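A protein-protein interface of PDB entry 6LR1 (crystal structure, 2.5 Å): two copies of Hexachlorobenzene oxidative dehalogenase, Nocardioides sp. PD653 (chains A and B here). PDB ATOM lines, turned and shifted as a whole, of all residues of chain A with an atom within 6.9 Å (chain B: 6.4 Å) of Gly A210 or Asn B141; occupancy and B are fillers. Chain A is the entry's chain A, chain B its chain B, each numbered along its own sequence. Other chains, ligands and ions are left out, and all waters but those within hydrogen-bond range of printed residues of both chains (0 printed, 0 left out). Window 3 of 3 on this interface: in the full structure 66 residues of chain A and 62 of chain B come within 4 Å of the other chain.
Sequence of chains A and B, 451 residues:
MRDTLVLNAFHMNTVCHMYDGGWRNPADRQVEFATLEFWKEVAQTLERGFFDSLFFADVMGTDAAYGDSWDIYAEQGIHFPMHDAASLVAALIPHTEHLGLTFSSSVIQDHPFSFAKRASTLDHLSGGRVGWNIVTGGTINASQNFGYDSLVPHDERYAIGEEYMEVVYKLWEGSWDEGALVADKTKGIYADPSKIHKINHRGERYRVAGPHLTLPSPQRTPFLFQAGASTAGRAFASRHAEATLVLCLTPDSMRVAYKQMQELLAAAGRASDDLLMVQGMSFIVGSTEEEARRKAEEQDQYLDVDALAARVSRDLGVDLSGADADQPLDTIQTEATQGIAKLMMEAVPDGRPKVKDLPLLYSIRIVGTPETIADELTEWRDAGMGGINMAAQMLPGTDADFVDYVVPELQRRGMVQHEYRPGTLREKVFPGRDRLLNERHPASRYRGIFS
O of Gln B144 sits at hydrogen-bond distance from N of Ala A209, at 3.2 Å.
The backbone carbonyl oxygen (O) of Gly A210 lies within hydrogen-bond range of the side-chain amide nitrogen (ND2) of Asn B141, 2.9 Å away.
The backbone NH of Gly A210 lies within hydrogen-bond range of the side-chain amide oxygen of Asn B145 (2.8 Å).
N of Ile A199 sits at hydrogen-bond distance from O of Ala A209 (2.6 Å).
The backbone NH of Asn A200 is in hydrogen-bond range of the backbone carbonyl oxygen of Ala A209 (3.0 Å).
The backbone carbonyl oxygen (O) of His A201 sits at hydrogen-bond distance from the backbone NH (N) of Val A208.
N of Thr B62 sits at hydrogen-bond distance from OD1 of Asn B141 (2.6 Å).
OD2 of Asp B63 sits at hydrogen-bond distance from N of Asn B141, 3.1 Å away.
The side-chain amide nitrogen of Asn B145 lies close to the backbone carbonyl oxygen of Asn B141 (3.2 Å).
CE2 of Phe A113 touches O of Met B60, 3.4 Å away.
CZ of Phe A113 touches ND2 of Asn B145, 3.2 Å away.
Gln B144 touches Val A208.
CG2 of Val A208 touches O of Asn B145, at 3.6 Å.
CB of Ala A209 touches OD1 of Asn B145, at 3.8 Å.
Thr B62 touches Pro A211.
Leu A213 touches Met B60.
Of the printed residues of chain B, Phe A113 touches Met B60 (3.4 Å) and Asn B145 (3.2 Å).
Gly A210 touches just these residues of chain B: Asn B141 (2.9 Å) and Asn B145 (2.8 Å).
Of the printed residues of chain A, Met B60 touches Phe A113 and Leu A213.
Printed residues of chain A within 4 Å of Asn B141: Gly A210.
Printed residues of chain A within 4 Å of Gln B144: Val A208 (3.6 Å) and Ala A209 (3.2 Å).
The nearest residue of chain B that does not touch Gly A210 is Gln B144 (5.4 Å).
Of the 14 printed residues of chain A, 6 touch a printed residue of chain B.
Of the 12 printed residues of chain B, 5 touch a printed residue of chain A.
Hydrophobic or aromatic side chains of chain B within 4 Å of the printed part of chain A: Met B60.
Among the printed residues, 10 pairs touch across the chains.
Among the printed residues, no Asp or Glu carboxylate lies within 4 Å of a Lys or Arg side-chain nitrogen of the other chain.
No position is printed for both chains.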
ATOM      1  N   PHE A 113      18.768  26.244   6.382  1.00  0.00           N
ATOM      2  CA  PHE A 113      19.079  25.018   7.130  1.00  0.00           C
ATOM      3  C   PHE A 113      17.901  24.595   7.920  1.00  0.00           C
ATOM      4  O   PHE A 113      17.601  23.397   7.912  1.00  0.00           O
ATOM      5  CB  PHE A 113      20.284  25.188   8.073  1.00  0.00           C
ATOM      6  CG  PHE A 113      20.702  23.927   8.785  1.00  0.00           C
ATOM      7  CD1 PHE A 113      21.603  23.074   8.224  1.00  0.00           C
ATOM      8  CD2 PHE A 113      20.192  23.617  10.038  1.00  0.00           C
ATOM      9  CE1 PHE A 113      21.996  21.935   8.891  1.00  0.00           C
ATOM     10  CE2 PHE A 113      20.571  22.469  10.714  1.00  0.00           C
ATOM     11  CZ  PHE A 113      21.467  21.625  10.136  1.00  0.00           C
ATOM     12  N   LEU A 171      22.099  20.494   0.884  1.00  0.00           N
ATOM     13  CA  LEU A 171      21.630  19.753   2.039  1.00  0.00           C
ATOM     14  C   LEU A 171      20.799  18.521   1.632  1.00  0.00           C
ATOM     15  O   LEU A 171      21.070  17.388   2.063  1.00  0.00           O
ATOM     16  CB  LEU A 171      20.805  20.688   2.944  1.00  0.00           C
ATOM     17  CG  LEU A 171      21.586  21.726   3.739  1.00  0.00           C
ATOM     18  CD1 LEU A 171      20.608  22.590   4.475  1.00  0.00           C
ATOM     19  CD2 LEU A 171      22.570  21.041   4.694  1.00  0.00           C
ATOM     20  N   SER A 175      24.484  16.144   0.853  1.00  0.00           N
ATOM     21  CA  SER A 175      25.031  15.881   2.179  1.00  0.00           C
ATOM     22  C   SER A 175      24.986  14.407   2.533  1.00  0.00           C
ATOM     23  O   SER A 175      25.952  13.923   3.140  1.00  0.00           O
ATOM     24  CB  SER A 175      24.338  16.728   3.250  1.00  0.00           C
ATOM     25  OG  SER A 175      24.823  16.410   4.551  1.00  0.00           O
ATOM     26  N   HIS A 197      28.148  13.927   4.886  1.00  0.00           N
ATOM     27  CA  HIS A 197      29.139  14.991   4.716  1.00  0.00           C
ATOM     28  C   HIS A 197      28.671  16.347   5.244  1.00  0.00           C
ATOM     29  O   HIS A 197      27.507  16.679   5.095  1.00  0.00           O
ATOM     30  CB  HIS A 197      29.437  15.169   3.202  1.00  0.00           C
ATOM     31  CG  HIS A 197      29.640  13.879   2.475  1.00  0.00           C
ATOM     32  ND1 HIS A 197      30.645  12.995   2.808  1.00  0.00           N
ATOM     33  CD2 HIS A 197      28.926  13.285   1.486  1.00  0.00           C
ATOM     34  CE1 HIS A 197      30.560  11.925   2.042  1.00  0.00           C
ATOM     35  NE2 HIS A 197      29.519  12.070   1.237  1.00  0.00           N
ATOM     36  N   LYS A 198      29.578  17.167   5.761  1.00  0.00           N
ATOM     37  CA  LYS A 198      29.307  18.623   5.843  1.00  0.00           C
ATOM     38  C   LYS A 198      29.165  19.204   4.442  1.00  0.00           C
ATOM     39  O   LYS A 198      29.681  18.632   3.465  1.00  0.00           O
ATOM     40  CB  LYS A 198      30.444  19.366   6.522  1.00  0.00           C
ATOM     41  CG  LYS A 198      30.554  19.114   7.984  1.00  0.00           C
ATOM     42  CD  LYS A 198      31.633  19.983   8.588  1.00  0.00           C
ATOM     43  CE  LYS A 198      32.331  19.251   9.724  1.00  0.00           C
ATOM     44  NZ  LYS A 198      32.761  20.198  10.788  1.00  0.00           N
ATOM     45  N   ILE A 199      28.489  20.329   4.327  1.00  0.00           N
ATOM     46  CA  ILE A 199      28.397  20.987   3.029  1.00  0.00           C
ATOM     47  C   ILE A 199      29.332  22.149   2.905  1.00  0.00           C
ATOM     48  O   ILE A 199      29.741  22.484   1.791  1.00  0.00           O
ATOM     49  CB  ILE A 199      26.968  21.368   2.664  1.00  0.00           C
ATOM     50  CG1 ILE A 199      26.360  22.452   3.592  1.00  0.00           C
ATOM     51  CG2 ILE A 199      26.127  20.114   2.720  1.00  0.00           C
ATOM     52  CD1 ILE A 199      25.183  23.215   2.968  1.00  0.00           C
ATOM     53  N   ASN A 200      29.724  22.740   4.037  1.00  0.00           N
ATOM     54  CA  ASN A 200      30.710  23.828   4.056  1.00  0.00           C
ATOM     55  C   ASN A 200      30.361  24.844   3.016  1.00  0.00           C
ATOM     56  O   ASN A 200      31.088  25.096   2.060  1.00  0.00           O
ATOM     57  CB  ASN A 200      32.111  23.275   3.895  1.00  0.00           C
ATOM     58  CG  ASN A 200      32.615  22.675   5.182  1.00  0.00           C
ATOM     59  OD1 ASN A 200      32.479  23.287   6.250  1.00  0.00           O
ATOM     60  ND2 ASN A 200      33.167  21.481   5.109  1.00  0.00           N
ATOM     61  N   HIS A 201      29.168  25.384   3.203  1.00  0.00           N
ATOM     62  CA  HIS A 201      28.670  26.365   2.291  1.00  0.00           C
ATOM     63  C   HIS A 201      29.133  27.747   2.762  1.00  0.00           C
ATOM     64  O   HIS A 201      28.789  28.168   3.898  1.00  0.00           O
ATOM     65  CB  HIS A 201      27.143  26.311   2.190  1.00  0.00           C
ATOM     66  CG  HIS A 201      26.598  27.470   1.468  1.00  0.00           C
ATOM     67  ND1 HIS A 201      26.566  27.524   0.093  1.00  0.00           N
ATOM     68  CD2 HIS A 201      26.227  28.695   1.911  1.00  0.00           C
ATOM     69  CE1 HIS A 201      26.112  28.717  -0.281  1.00  0.00           C
ATOM     70  NE2 HIS A 201      25.942  29.463   0.802  1.00  0.00           N
ATOM     71  N   VAL A 208      27.056  27.845   6.222  1.00  0.00           N
ATOM     72  CA  VAL A 208      26.318  26.692   6.728  1.00  0.00           C
ATOM     73  C   VAL A 208      27.194  25.459   6.661  1.00  0.00           C
ATOM     74  O   VAL A 208      27.441  24.934   5.577  1.00  0.00           O
ATOM     75  CB  VAL A 208      25.027  26.396   5.875  1.00  0.00           C
ATOM     76  CG1 VAL A 208      24.309  25.147   6.415  1.00  0.00           C
ATOM     77  CG2 VAL A 208      24.080  27.590   5.827  1.00  0.00           C
ATOM     78  N   ALA A 209      27.620  24.975   7.803  1.00  0.00           N
ATOM     79  CA  ALA A 209      28.445  23.795   7.845  1.00  0.00           C
ATOM     80  C   ALA A 209      27.772  22.482   7.348  1.00  0.00           C
ATOM     81  O   ALA A 209      28.339  21.737   6.512  1.00  0.00           O
ATOM     82  CB  ALA A 209      28.958  23.620   9.258  1.00  0.00           C
ATOM     83  N   GLY A 210      26.576  22.196   7.874  1.00  0.00           N
ATOM     84  CA  GLY A 210      25.969  20.897   7.676  1.00  0.00           C
ATOM     85  C   GLY A 210      26.667  19.917   8.612  1.00  0.00           C
ATOM     86  O   GLY A 210      27.338  20.332   9.536  1.00  0.00           O
ATOM     87  N   PRO A 211      26.516  18.610   8.432  1.00  0.00           N
ATOM     88  CA  PRO A 211      25.662  17.972   7.424  1.00  0.00           C
ATOM     89  C   PRO A 211      24.194  18.257   7.614  1.00  0.00           C
ATOM     90  O   PRO A 211      23.811  18.805   8.650  1.00  0.00           O
ATOM     91  CB  PRO A 211      25.927  16.502   7.661  1.00  0.00           C
ATOM     92  CG  PRO A 211      26.270  16.411   9.103  1.00  0.00           C
ATOM     93  CD  PRO A 211      26.783  17.732   9.576  1.00  0.00           C
ATOM     94  N   HIS A 212      23.388  17.908   6.602  1.00  0.00           N
ATOM     95  CA  HIS A 212      21.921  17.823   6.737  1.00  0.00           C
ATOM     96  C   HIS A 212      21.563  16.843   7.836  1.00  0.00           C
ATOM     97  O   HIS A 212      22.162  15.784   7.878  1.00  0.00           O
ATOM     98  CB  HIS A 212      21.276  17.341   5.433  1.00  0.00           C
ATOM     99  CG  HIS A 212      19.782  17.510   5.386  1.00  0.00           C
ATOM    100  ND1 HIS A 212      19.148  18.681   5.738  1.00  0.00           N
ATOM    101  CD2 HIS A 212      18.804  16.659   4.994  1.00  0.00           C
ATOM    102  CE1 HIS A 212      17.843  18.541   5.574  1.00  0.00           C
ATOM    103  NE2 HIS A 212      17.607  17.325   5.117  1.00  0.00           N
ATOM    104  N   LEU A 213      20.607  17.180   8.711  1.00  0.00           N
ATOM    105  CA  LEU A 213      20.276  16.305   9.826  1.00  0.00           C
ATOM    106  C   LEU A 213      19.350  15.129   9.527  1.00  0.00           C
ATOM    107  O   LEU A 213      19.300  14.235  10.333  1.00  0.00           O
ATOM    108  CB  LEU A 213      19.686  17.105  10.969  1.00  0.00           C
ATOM    109  CG  LEU A 213      20.700  18.038  11.626  1.00  0.00           C
ATOM    110  CD1 LEU A 213      20.013  19.216  12.257  1.00  0.00           C
ATOM    111  CD2 LEU A 213      21.476  17.284  12.668  1.00  0.00           C
ATOM    112  N   MET B  60      19.779  21.122  16.593  1.00  0.00           N
ATOM    113  CA  MET B  60      20.060  21.729  15.311  1.00  0.00           C
ATOM    114  C   MET B  60      21.468  21.539  14.792  1.00  0.00           C
ATOM    115  O   MET B  60      21.868  22.163  13.809  1.00  0.00           O
ATOM    116  CB  MET B  60      19.709  23.217  15.375  1.00  0.00           C
ATOM    117  CG  MET B  60      18.221  23.534  15.605  1.00  0.00           C
ATOM    118  SD  MET B  60      16.993  22.867  14.414  1.00  0.00           S
ATOM    119  CE  MET B  60      17.447  23.541  12.804  1.00  0.00           C
ATOM    120  N   GLY B  61      22.205  20.608  15.377  1.00  0.00           N
ATOM    121  CA  GLY B  61      23.588  20.294  14.946  1.00  0.00           C
ATOM    122  C   GLY B  61      24.027  18.926  15.421  1.00  0.00           C
ATOM    123  O   GLY B  61      23.369  18.323  16.238  1.00  0.00           O
ATOM    124  N   THR B  62      25.143  18.436  14.890  1.00  0.00           N
ATOM    125  CA  THR B  62      25.830  17.227  15.377  1.00  0.00           C
ATOM    126  C   THR B  62      27.339  17.515  15.475  1.00  0.00           C
ATOM    127  O   THR B  62      27.922  18.115  14.582  1.00  0.00           O
ATOM    128  CB  THR B  62      25.566  16.025  14.465  1.00  0.00           C
ATOM    129  OG1 THR B  62      26.099  14.824  15.047  1.00  0.00           O
ATOM    130  CG2 THR B  62      26.165  16.252  13.096  1.00  0.00           C
ATOM    131  N   ASP B  63      27.964  17.089  16.570  1.00  0.00           N
ATOM    132  CA  ASP B  63      29.338  17.488  16.885  1.00  0.00           C
ATOM    133  C   ASP B  63      30.254  16.300  17.152  1.00  0.00           C
ATOM    134  O   ASP B  63      29.889  15.360  17.886  1.00  0.00           O
ATOM    135  CB  ASP B  63      29.331  18.445  18.071  1.00  0.00           C
ATOM    136  CG  ASP B  63      29.152  19.866  17.648  1.00  0.00           C
ATOM    137  OD1 ASP B  63      29.908  20.339  16.770  1.00  0.00           O
ATOM    138  OD2 ASP B  63      28.283  20.537  18.195  1.00  0.00           O
ATOM    139  N   THR B 139      25.124  23.822  20.418  1.00  0.00           N
ATOM    140  CA  THR B 139      26.291  23.010  20.181  1.00  0.00           C
ATOM    141  C   THR B 139      27.062  23.774  19.113  1.00  0.00           C
ATOM    142  O   THR B 139      26.505  24.644  18.446  1.00  0.00           O
ATOM    143  CB  THR B 139      25.795  21.599  19.770  1.00  0.00           C
ATOM    144  OG1 THR B 139      26.777  20.596  20.035  1.00  0.00           O
ATOM    145  CG2 THR B 139      25.331  21.531  18.314  1.00  0.00           C
ATOM    146  N   ILE B 140      28.353  23.514  18.980  1.00  0.00           N
ATOM    147  CA  ILE B 140      29.182  24.292  18.037  1.00  0.00           C
ATOM    148  C   ILE B 140      28.603  24.179  16.597  1.00  0.00           C
ATOM    149  O   ILE B 140      28.455  25.188  15.877  1.00  0.00           O
ATOM    150  CB  ILE B 140      30.691  23.866  18.102  1.00  0.00           C
ATOM    151  CG1 ILE B 140      31.290  24.229  19.480  1.00  0.00           C
ATOM    152  CG2 ILE B 140      31.505  24.548  17.008  1.00  0.00           C
ATOM    153  CD1 ILE B 140      32.579  23.519  19.841  1.00  0.00           C
ATOM    154  N   ASN B 141      28.237  22.947  16.215  1.00  0.00           N
ATOM    155  CA  ASN B 141      27.773  22.644  14.861  1.00  0.00           C
ATOM    156  C   ASN B 141      26.542  23.435  14.506  1.00  0.00           C
ATOM    157  O   ASN B 141      26.459  23.906  13.389  1.00  0.00           O
ATOM    158  CB  ASN B 141      27.471  21.157  14.693  1.00  0.00           C
ATOM    159  CG  ASN B 141      27.092  20.784  13.269  1.00  0.00           C
ATOM    160  OD1 ASN B 141      26.145  20.052  13.074  1.00  0.00           O
ATOM    161  ND2 ASN B 141      27.849  21.246  12.281  1.00  0.00           N
ATOM    162  N   ALA B 142      25.625  23.582  15.470  1.00  0.00           N
ATOM    163  CA  ALA B 142      24.337  24.286  15.315  1.00  0.00           C
ATOM    164  C   ALA B 142      24.643  25.744  15.048  1.00  0.00           C
ATOM    165  O   ALA B 142      24.064  26.345  14.156  1.00  0.00           O
ATOM    166  CB  ALA B 142      23.471  24.156  16.578  1.00  0.00           C
ATOM    167  N   SER B 143      25.597  26.306  15.789  1.00  0.00           N
ATOM    168  CA  SER B 143      26.007  27.690  15.541  1.00  0.00           C
ATOM    169  C   SER B 143      26.453  27.840  14.100  1.00  0.00           C
ATOM    170  O   SER B 143      25.935  28.680  13.327  1.00  0.00           O
ATOM    171  CB  SER B 143      27.096  28.123  16.508  1.00  0.00           C
ATOM    172  OG  SER B 143      26.523  28.445  17.760  1.00  0.00           O
ATOM    173  N   GLN B 144      27.381  26.977  13.736  1.00  0.00           N
ATOM    174  CA  GLN B 144      27.916  26.973  12.384  1.00  0.00           C
ATOM    175  C   GLN B 144      26.881  26.657  11.304  1.00  0.00           C
ATOM    176  O   GLN B 144      27.052  27.089  10.179  1.00  0.00           O
ATOM    177  CB  GLN B 144      29.114  26.041  12.308  1.00  0.00           C
ATOM    178  CG  GLN B 144      30.290  26.590  13.113  1.00  0.00           C
ATOM    179  CD  GLN B 144      31.535  25.710  13.072  1.00  0.00           C
ATOM    180  OE1 GLN B 144      32.612  26.119  13.532  1.00  0.00           O
ATOM    181  NE2 GLN B 144      31.393  24.496  12.527  1.00  0.00           N
ATOM    182  N   ASN B 145      25.802  25.947  11.639  1.00  0.00           N
ATOM    183  CA  ASN B 145      24.675  25.766  10.686  1.00  0.00           C
ATOM    184  C   ASN B 145      23.908  27.050  10.389  1.00  0.00           C
ATOM    185  O   ASN B 145      23.350  27.177   9.319  1.00  0.00           O
ATOM    186  CB  ASN B 145      23.731  24.647  11.128  1.00  0.00           C
ATOM    187  CG  ASN B 145      24.399  23.294  11.055  1.00  0.00           C
ATOM    188  OD1 ASN B 145      25.286  23.075  10.221  1.00  0.00           O
ATOM    189  ND2 ASN B 145      24.013  22.386  11.936  1.00  0.00           N
ATOM    190  N   PHE B 146      23.944  28.007  11.321  1.00  0.00           N
ATOM    191  CA  PHE B 146      23.338  29.346  11.151  1.00  0.00           C
ATOM    192  C   PHE B 146      24.370  30.484  10.976  1.00  0.00           C
ATOM    193  O   PHE B 146      24.079  31.614  11.312  1.00  0.00           O
ATOM    194  CB  PHE B 146      22.374  29.611  12.330  1.00  0.00           C
ATOM    195  CG  PHE B 146      21.281  28.587  12.441  1.00  0.00           C
ATOM    196  CD1 PHE B 146      21.472  27.419  13.176  1.00  0.00           C
ATOM    197  CD2 PHE B 146      20.078  28.764  11.757  1.00  0.00           C
ATOM    198  CE1 PHE B 146      20.492  26.471  13.276  1.00  0.00           C
ATOM    199  CE2 PHE B 146      19.073  27.814  11.834  1.00  0.00           C
ATOM    200  CZ  PHE B 146      19.274  26.657  12.587  1.00  0.00           C
